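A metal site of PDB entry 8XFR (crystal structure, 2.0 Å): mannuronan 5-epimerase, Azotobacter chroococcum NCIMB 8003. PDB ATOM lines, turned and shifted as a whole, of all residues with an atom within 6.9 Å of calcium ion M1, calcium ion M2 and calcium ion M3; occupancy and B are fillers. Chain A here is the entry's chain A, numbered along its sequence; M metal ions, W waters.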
ATOM      1  N   ASN A 322      17.785  -0.300  37.661  1.00  0.00           N
ATOM      2  CA  ASN A 322      18.119   0.677  38.704  1.00  0.00           C
ATOM      3  C   ASN A 322      19.411   0.319  39.419  1.00  0.00           C
ATOM      4  O   ASN A 322      19.474   0.240  40.638  1.00  0.00           O
ATOM      5  CB  ASN A 322      16.971   0.786  39.697  1.00  0.00           C
ATOM      6  CG  ASN A 322      15.717   1.324  39.038  1.00  0.00           C
ATOM      7  OD1 ASN A 322      15.789   2.302  38.267  1.00  0.00           O
ATOM      8  ND2 ASN A 322      14.578   0.625  39.240  1.00  0.00           N
ATOM      9  N   SER A 338      22.219  -3.430  32.311  1.00  0.00           N
ATOM     10  CA  SER A 338      20.974  -3.068  32.989  1.00  0.00           C
ATOM     11  C   SER A 338      19.927  -2.730  31.927  1.00  0.00           C
ATOM     12  O   SER A 338      20.185  -2.814  30.726  1.00  0.00           O
ATOM     13  CB  SER A 338      21.212  -1.931  33.986  1.00  0.00           C
ATOM     14  OG  SER A 338      20.118  -1.845  34.883  1.00  0.00           O
ATOM     15  N   SER A 339      18.764  -2.254  32.378  1.00  0.00           N
ATOM     16  CA  SER A 339      17.590  -2.120  31.519  1.00  0.00           C
ATOM     17  C   SER A 339      16.932  -0.768  31.810  1.00  0.00           C
ATOM     18  O   SER A 339      17.594   0.193  32.208  1.00  0.00           O
ATOM     19  CB  SER A 339      16.675  -3.328  31.710  1.00  0.00           C
ATOM     20  OG  SER A 339      17.256  -4.490  31.134  1.00  0.00           O
ATOM     21  N   GLU A 340      15.632  -0.665  31.494  1.00  0.00           N
ATOM     22  CA  GLU A 340      14.874   0.586  31.553  1.00  0.00           C
ATOM     23  C   GLU A 340      15.124   1.366  32.869  1.00  0.00           C
ATOM     24  O   GLU A 340      15.247   0.774  33.952  1.00  0.00           O
ATOM     25  CB  GLU A 340      13.383   0.308  31.403  1.00  0.00           C
ATOM     26  CG  GLU A 340      12.523   1.599  31.519  1.00  0.00           C
ATOM     27  CD  GLU A 340      12.867   2.678  30.456  1.00  0.00           C
ATOM     28  OE1 GLU A 340      12.285   2.608  29.342  1.00  0.00           O
ATOM     29  OE2 GLU A 340      13.737   3.579  30.712  1.00  0.00           O
ATOM     30  N   GLY A 341      15.203   2.687  32.752  1.00  0.00           N
ATOM     31  CA  GLY A 341      15.531   3.541  33.882  1.00  0.00           C
ATOM     32  C   GLY A 341      17.008   3.944  33.873  1.00  0.00           C
ATOM     33  O   GLY A 341      17.823   3.431  33.102  1.00  0.00           O
ATOM     34  N   ARG A 342      17.346   4.867  34.765  1.00  0.00           N
ATOM     35  CA  ARG A 342      18.680   5.453  34.784  1.00  0.00           C
ATOM     36  C   ARG A 342      19.637   4.544  35.541  1.00  0.00           C
ATOM     37  O   ARG A 342      19.405   4.238  36.717  1.00  0.00           O
ATOM     38  CB  ARG A 342      18.639   6.836  35.447  1.00  0.00           C
ATOM     39  CG  ARG A 342      19.989   7.454  35.711  1.00  0.00           C
ATOM     40  CD  ARG A 342      19.894   8.989  35.546  1.00  0.00           C
ATOM     41  NE  ARG A 342      21.158   9.634  35.876  1.00  0.00           N
ATOM     42  CZ  ARG A 342      22.226   9.650  35.078  1.00  0.00           C
ATOM     43  NH1 ARG A 342      22.203   9.046  33.894  1.00  0.00           N
ATOM     44  NH2 ARG A 342      23.317  10.305  35.472  1.00  0.00           N
ATOM     45  N   ASP A 343      20.710   4.118  34.881  1.00  0.00           N
ATOM     46  CA  ASP A 343      21.775   3.360  35.514  1.00  0.00           C
ATOM     47  C   ASP A 343      23.056   4.170  35.486  1.00  0.00           C
ATOM     48  O   ASP A 343      23.275   4.963  34.580  1.00  0.00           O
ATOM     49  CB  ASP A 343      21.985   2.028  34.756  1.00  0.00           C
ATOM     50  CG  ASP A 343      20.741   1.171  34.805  1.00  0.00           C
ATOM     51  OD1 ASP A 343      20.545   0.509  35.851  1.00  0.00           O
ATOM     52  OD2 ASP A 343      19.940   1.170  33.839  1.00  0.00           O
ATOM     53  N   LEU A 345      26.933   3.102  35.631  1.00  0.00           N
ATOM     54  CA  LEU A 345      27.756   1.899  35.546  1.00  0.00           C
ATOM     55  C   LEU A 345      29.201   2.322  35.318  1.00  0.00           C
ATOM     56  O   LEU A 345      29.523   2.873  34.262  1.00  0.00           O
ATOM     57  CB  LEU A 345      27.255   0.979  34.419  1.00  0.00           C
ATOM     58  CG  LEU A 345      25.759   0.624  34.508  1.00  0.00           C
ATOM     59  CD1 LEU A 345      25.270  -0.153  33.262  1.00  0.00           C
ATOM     60  CD2 LEU A 345      25.477  -0.212  35.760  1.00  0.00           C
ATOM     61  N   ASP A 355      26.482  -1.845  29.350  1.00  0.00           N
ATOM     62  CA  ASP A 355      25.255  -1.620  28.591  1.00  0.00           C
ATOM     63  C   ASP A 355      24.178  -1.215  29.575  1.00  0.00           C
ATOM     64  O   ASP A 355      23.642  -2.057  30.285  1.00  0.00           O
ATOM     65  CB  ASP A 355      24.838  -2.880  27.826  1.00  0.00           C
ATOM     66  CG  ASP A 355      23.706  -2.607  26.806  1.00  0.00           C
ATOM     67  OD1 ASP A 355      23.015  -1.545  26.879  1.00  0.00           O
ATOM     68  OD2 ASP A 355      23.517  -3.465  25.902  1.00  0.00           O
ATOM     69  N   GLY A 356      23.816   0.058  29.565  1.00  0.00           N
ATOM     70  CA  GLY A 356      22.712   0.444  30.422  1.00  0.00           C
ATOM     71  C   GLY A 356      21.316   0.172  29.874  1.00  0.00           C
ATOM     72  O   GLY A 356      20.344   0.407  30.592  1.00  0.00           O
ATOM     73  N   GLY A 357      21.173  -0.338  28.647  1.00  0.00           N
ATOM     74  CA  GLY A 357      19.818  -0.643  28.197  1.00  0.00           C
ATOM     75  C   GLY A 357      18.990   0.623  27.974  1.00  0.00           C
ATOM     76  O   GLY A 357      19.512   1.701  27.717  1.00  0.00           O
ATOM     77  N   ALA A 358      17.663   0.501  28.087  1.00  0.00           N
ATOM     78  CA  ALA A 358      16.825   1.670  27.912  1.00  0.00           C
ATOM     79  C   ALA A 358      17.067   2.683  29.033  1.00  0.00           C
ATOM     80  O   ALA A 358      17.650   2.379  30.076  1.00  0.00           O
ATOM     81  CB  ALA A 358      15.353   1.269  27.843  1.00  0.00           C
ATOM     82  N   GLY A 359      16.656   3.933  28.789  1.00  0.00           N
ATOM     83  CA  GLY A 359      16.817   4.999  29.764  1.00  0.00           C
ATOM     84  C   GLY A 359      18.130   5.764  29.630  1.00  0.00           C
ATOM     85  O   GLY A 359      19.050   5.383  28.909  1.00  0.00           O
ATOM     86  N   ARG A 360      18.222   6.866  30.384  1.00  0.00           N
ATOM     87  CA  ARG A 360      19.388   7.745  30.352  1.00  0.00           C
ATOM     88  C   ARG A 360      20.460   7.235  31.294  1.00  0.00           C
ATOM     89  O   ARG A 360      20.357   7.391  32.519  1.00  0.00           O
ATOM     90  CB  ARG A 360      18.996   9.182  30.718  1.00  0.00           C
ATOM     91  CG  ARG A 360      20.115  10.165  30.406  1.00  0.00           C
ATOM     92  CD  ARG A 360      19.718  11.610  30.700  1.00  0.00           C
ATOM     93  NE  ARG A 360      19.647  11.900  32.130  1.00  0.00           N
ATOM     94  CZ  ARG A 360      20.683  12.179  32.916  1.00  0.00           C
ATOM     95  NH1 ARG A 360      21.922  12.230  32.439  1.00  0.00           N
ATOM     96  NH2 ARG A 360      20.466  12.405  34.206  1.00  0.00           N
ATOM     97  N   ASP A 361      21.509   6.627  30.743  1.00  0.00           N
ATOM     98  CA  ASP A 361      22.536   6.000  31.557  1.00  0.00           C
ATOM     99  C   ASP A 361      23.841   6.766  31.458  1.00  0.00           C
ATOM    100  O   ASP A 361      24.150   7.383  30.435  1.00  0.00           O
ATOM    101  CB  ASP A 361      22.740   4.545  31.109  1.00  0.00           C
ATOM    102  CG  ASP A 361      21.442   3.785  31.079  1.00  0.00           C
ATOM    103  OD1 ASP A 361      20.738   3.766  32.102  1.00  0.00           O
ATOM    104  OD2 ASP A 361      21.073   3.256  30.025  1.00  0.00           O
ATOM    105  N   THR A 362      24.610   6.726  32.536  1.00  0.00           N
ATOM    106  CA  THR A 362      25.946   7.288  32.536  1.00  0.00           C
ATOM    107  C   THR A 362      26.936   6.146  32.733  1.00  0.00           C
ATOM    108  O   THR A 362      26.856   5.429  33.733  1.00  0.00           O
ATOM    109  CB  THR A 362      26.082   8.349  33.626  1.00  0.00           C
ATOM    110  OG1 THR A 362      25.161   9.420  33.333  1.00  0.00           O
ATOM    111  CG2 THR A 362      27.494   8.884  33.661  1.00  0.00           C
ATOM    112  N   LEU A 363      27.875   6.007  31.802  1.00  0.00           N
ATOM    113  CA  LEU A 363      28.791   4.875  31.767  1.00  0.00           C
ATOM    114  C   LEU A 363      30.223   5.362  31.794  1.00  0.00           C
ATOM    115  O   LEU A 363      30.559   6.383  31.182  1.00  0.00           O
ATOM    116  CB  LEU A 363      28.585   4.013  30.513  1.00  0.00           C
ATOM    117  CG  LEU A 363      27.135   3.768  30.088  1.00  0.00           C
ATOM    118  CD1 LEU A 363      27.044   3.368  28.619  1.00  0.00           C
ATOM    119  CD2 LEU A 363      26.523   2.670  30.938  1.00  0.00           C
ATOM    120  N   PHE A 374      25.453  -0.531  22.712  1.00  0.00           N
ATOM    121  CA  PHE A 374      24.116   0.016  22.521  1.00  0.00           C
ATOM    122  C   PHE A 374      23.388  -0.968  21.638  1.00  0.00           C
ATOM    123  O   PHE A 374      23.688  -1.077  20.442  1.00  0.00           O
ATOM    124  CB  PHE A 374      24.184   1.418  21.928  1.00  0.00           C
ATOM    125  CG  PHE A 374      24.909   2.356  22.809  1.00  0.00           C
ATOM    126  CD1 PHE A 374      26.298   2.379  22.812  1.00  0.00           C
ATOM    127  CD2 PHE A 374      24.218   3.142  23.711  1.00  0.00           C
ATOM    128  CE1 PHE A 374      26.973   3.202  23.657  1.00  0.00           C
ATOM    129  CE2 PHE A 374      24.885   3.963  24.563  1.00  0.00           C
ATOM    130  CZ  PHE A 374      26.267   4.002  24.549  1.00  0.00           C
ATOM    131  N   ALA A 375      22.486  -1.721  22.255  1.00  0.00           N
ATOM    132  CA  ALA A 375      21.829  -2.850  21.608  1.00  0.00           C
ATOM    133  C   ALA A 375      20.600  -2.464  20.820  1.00  0.00           C
ATOM    134  O   ALA A 375      20.111  -3.283  20.037  1.00  0.00           O
ATOM    135  CB  ALA A 375      21.431  -3.875  22.676  1.00  0.00           C
ATOM    136  N   ASP A 376      20.075  -1.247  20.991  1.00  0.00           N
ATOM    137  CA  ASP A 376      18.787  -0.851  20.457  1.00  0.00           C
ATOM    138  C   ASP A 376      18.826   0.656  20.214  1.00  0.00           C
ATOM    139  O   ASP A 376      19.363   1.403  21.036  1.00  0.00           O
ATOM    140  CB  ASP A 376      17.665  -1.239  21.439  1.00  0.00           C
ATOM    141  CG  ASP A 376      16.294  -1.062  20.868  1.00  0.00           C
ATOM    142  OD1 ASP A 376      15.896   0.080  20.524  1.00  0.00           O
ATOM    143  OD2 ASP A 376      15.589  -2.064  20.767  1.00  0.00           O
ATOM    144  N   ARG A 377      18.258   1.099  19.096  1.00  0.00           N
ATOM    145  CA  ARG A 377      18.268   2.528  18.790  1.00  0.00           C
ATOM    146  C   ARG A 377      17.498   3.342  19.822  1.00  0.00           C
ATOM    147  O   ARG A 377      17.761   4.543  19.983  1.00  0.00           O
ATOM    148  CB  ARG A 377      17.681   2.767  17.392  1.00  0.00           C
ATOM    149  CG  ARG A 377      18.678   2.570  16.263  1.00  0.00           C
ATOM    150  CD  ARG A 377      18.017   2.681  14.887  1.00  0.00           C
ATOM    151  NE  ARG A 377      18.956   2.271  13.842  1.00  0.00           N
ATOM    152  CZ  ARG A 377      19.000   2.773  12.613  1.00  0.00           C
ATOM    153  NH1 ARG A 377      18.173   3.728  12.225  1.00  0.00           N
ATOM    154  NH2 ARG A 377      19.904   2.298  11.754  1.00  0.00           N
ATOM    155  N   GLN A 378      16.563   2.722  20.540  1.00  0.00           N
ATOM    156  CA  GLN A 378      15.798   3.403  21.554  1.00  0.00           C
ATOM    157  C   GLN A 378      16.470   3.353  22.930  1.00  0.00           C
ATOM    158  O   GLN A 378      15.861   3.748  23.929  1.00  0.00           O
ATOM    159  CB  GLN A 378      14.382   2.795  21.636  1.00  0.00           C
ATOM    160  CG  GLN A 378      13.506   2.982  20.386  1.00  0.00           C
ATOM    161  CD  GLN A 378      13.435   4.422  19.870  1.00  0.00           C
ATOM    162  OE1 GLN A 378      12.951   5.338  20.582  1.00  0.00           O
ATOM    163  NE2 GLN A 378      13.913   4.641  18.634  1.00  0.00           N
ATOM    164  N   ASP A 379      17.706   2.888  23.008  1.00  0.00           N
ATOM    165  CA  ASP A 379      18.374   2.844  24.297  1.00  0.00           C
ATOM    166  C   ASP A 379      19.094   4.142  24.630  1.00  0.00           C
ATOM    167  O   ASP A 379      19.468   4.336  25.793  1.00  0.00           O
ATOM    168  CB  ASP A 379      19.358   1.684  24.317  1.00  0.00           C
ATOM    169  CG  ASP A 379      18.641   0.319  24.415  1.00  0.00           C
ATOM    170  OD1 ASP A 379      17.395   0.301  24.615  1.00  0.00           O
ATOM    171  OD2 ASP A 379      19.313  -0.703  24.293  1.00  0.00           O
ATOM    172  N   SER A 380      19.254   5.031  23.652  1.00  0.00           N
ATOM    173  CA  SER A 380      19.927   6.320  23.842  1.00  0.00           C
ATOM    174  C   SER A 380      19.434   7.205  22.717  1.00  0.00           C
ATOM    175  O   SER A 380      19.778   6.945  21.563  1.00  0.00           O
ATOM    176  CB  SER A 380      21.452   6.155  23.810  1.00  0.00           C
ATOM    177  OG  SER A 380      22.134   7.336  24.215  1.00  0.00           O
ATOM    178  N   PHE A 381      18.600   8.205  23.029  1.00  0.00           N
ATOM    179  CA  PHE A 381      17.871   8.930  21.989  1.00  0.00           C
ATOM    180  C   PHE A 381      17.386  10.290  22.485  1.00  0.00           C
ATOM    181  O   PHE A 381      17.213  10.533  23.682  1.00  0.00           O
ATOM    182  CB  PHE A 381      16.682   8.104  21.472  1.00  0.00           C
ATOM    183  CG  PHE A 381      15.502   8.070  22.412  1.00  0.00           C
ATOM    184  CD1 PHE A 381      15.449   7.138  23.449  1.00  0.00           C
ATOM    185  CD2 PHE A 381      14.442   8.956  22.262  1.00  0.00           C
ATOM    186  CE1 PHE A 381      14.368   7.104  24.313  1.00  0.00           C
ATOM    187  CE2 PHE A 381      13.354   8.920  23.133  1.00  0.00           C
ATOM    188  CZ  PHE A 381      13.321   7.996  24.162  1.00  0.00           C
ATOM    189  N   ARG A 390      17.118  10.938  28.150  1.00  0.00           N
ATOM    190  CA  ARG A 390      17.193   9.639  27.499  1.00  0.00           C
ATOM    191  C   ARG A 390      18.428   9.514  26.596  1.00  0.00           C
ATOM    192  O   ARG A 390      18.585   8.485  25.953  1.00  0.00           O
ATOM    193  CB  ARG A 390      15.928   9.299  26.693  1.00  0.00           C
ATOM    194  CG  ARG A 390      14.563   9.427  27.420  1.00  0.00           C
ATOM    195  CD  ARG A 390      14.527   9.009  28.888  1.00  0.00           C
ATOM    196  NE  ARG A 390      14.785  10.082  29.844  1.00  0.00           N
ATOM    197  CZ  ARG A 390      13.958  11.096  30.083  1.00  0.00           C
ATOM    198  NH1 ARG A 390      12.879  11.302  29.345  1.00  0.00           N
ATOM    199  NH2 ARG A 390      14.230  11.928  31.086  1.00  0.00           N
ATOM    200  N   VAL A 391      19.314  10.500  26.554  1.00  0.00           N
ATOM    201  CA  VAL A 391      20.600  10.343  25.872  1.00  0.00           C
ATOM    202  C   VAL A 391      21.667   9.882  26.865  1.00  0.00           C
ATOM    203  O   VAL A 391      21.971  10.591  27.835  1.00  0.00           O
ATOM    204  CB  VAL A 391      21.018  11.626  25.141  1.00  0.00           C
ATOM    205  CG1 VAL A 391      22.423  11.469  24.555  1.00  0.00           C
ATOM    206  CG2 VAL A 391      20.013  11.919  24.023  1.00  0.00           C
ATOM    207  N   ASP A 392      22.253   8.714  26.610  1.00  0.00           N
ATOM    208  CA  ASP A 392      23.364   8.213  27.424  1.00  0.00           C
ATOM    209  C   ASP A 392      24.590   9.103  27.285  1.00  0.00           C
ATOM    210  O   ASP A 392      24.840   9.677  26.223  1.00  0.00           O
ATOM    211  CB  ASP A 392      23.778   6.807  26.976  1.00  0.00           C
ATOM    212  CG  ASP A 392      22.779   5.731  27.347  1.00  0.00           C
ATOM    213  OD1 ASP A 392      21.715   6.060  27.920  1.00  0.00           O
ATOM    214  OD2 ASP A 392      23.097   4.555  27.093  1.00  0.00           O
HETATM  215 CA    CA M   1      20.557   3.946  27.798  1.00  0.00          CA
HETATM  216 CA    CA M   2      19.103   2.019  31.788  1.00  0.00          CA
HETATM  217 CA    CA M   3      16.674  -2.152  24.016  1.00  0.00          CA
HETATM  218  O   HOH W   1      18.451  -3.384  24.976  1.00  0.00           O
HETATM  219  O   HOH W   2      21.924   2.387  26.427  1.00  0.00           O
HETATM  220  O   HOH W   3      14.991  -1.599  25.590  1.00  0.00           O
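The backbone carbonyl oxygen (O) of Asp 343 is in hydrogen-bond range of the backbone NH (N) of Thr 362. OD1 of Asp 355 is in hydrogen-bond range of N of Gly 357 (2.8 Å). N of Asn 322 sits at hydrogen-bond distance from OD1 of Asp 343 (3.4 Å). The side-chain hydroxyl (OG) of Ser 338 lies within hydrogen-bond range of the side-chain carboxylate (OD1) of Asp 343 (2.6 Å). The side-chain carboxylate (OD1) of Asp 376 lies within hydrogen-bond range of the backbone NH (N) of Gln 378 (2.7 Å). The side-chain hydroxyl of Ser 380 is in hydrogen-bond range of the backbone NH of Asp 392 (2.8 Å). N of Gly 357 sits close to O of Ser 338 (3.4 Å). N of Asp 376 lies close to OD2 of Asp 379, at 3.4 Å.
Of the 28 residues printed, 6 come within 4 Å of calcium ion M1.
Within 4 Å of calcium ion M2: Ser 339, Gly 341, Asp 343, Gly 356, Ala 358 and Asp 361.
Asp 376 touches calcium ion M3 (CB to CA, 2.9 Å). Two residues have an atom within 4 Å of calcium ion M3: Asp 376 and Asp 379. Along chain A the residues within 4 Å of calcium ion M3 span positions 376 to 379. The nearest printed residue that does not touch calcium ion M3 is Ala 358 (5.0 Å).
Calcium ion M1 is bound by the backbone carbonyl oxygen (O) of Asp 379 (2.3 Å), the backbone carbonyl oxygen (O) of Gly 359 (2.4 Å), the side-chain carboxylate (OD2) of Asp 361 (2.4 Å), the side-chain carboxylate (OD1) of Asp 392 (2.4 Å), the backbone carbonyl oxygen (O) of Gly 357 (2.5 Å), water W2 (2.5 Å) and the side-chain carboxylate (OD2) of Asp 392 (2.7 Å).
Calcium ion M2 is bound by O of Ala 358, O of Gly 341, O of Gly 356, OD2 of Asp 343, O of Ser 339 and OD1 of Asp 361. Calcium ion M2 has six donor atoms within binding distance. Slightly farther from calcium ion M2 lies OD2 of Asp 361 (2.9 Å).
Calcium ion M3 is bound by water W1 (2.4 Å). Calcium ion M3 is bound by water W3 (2.4 Å). OD1 of Asp 379 binds calcium ion M3, 2.6 Å away. Slightly farther from calcium ion M3 lies OD2 of Asp 379 (3.0 Å).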
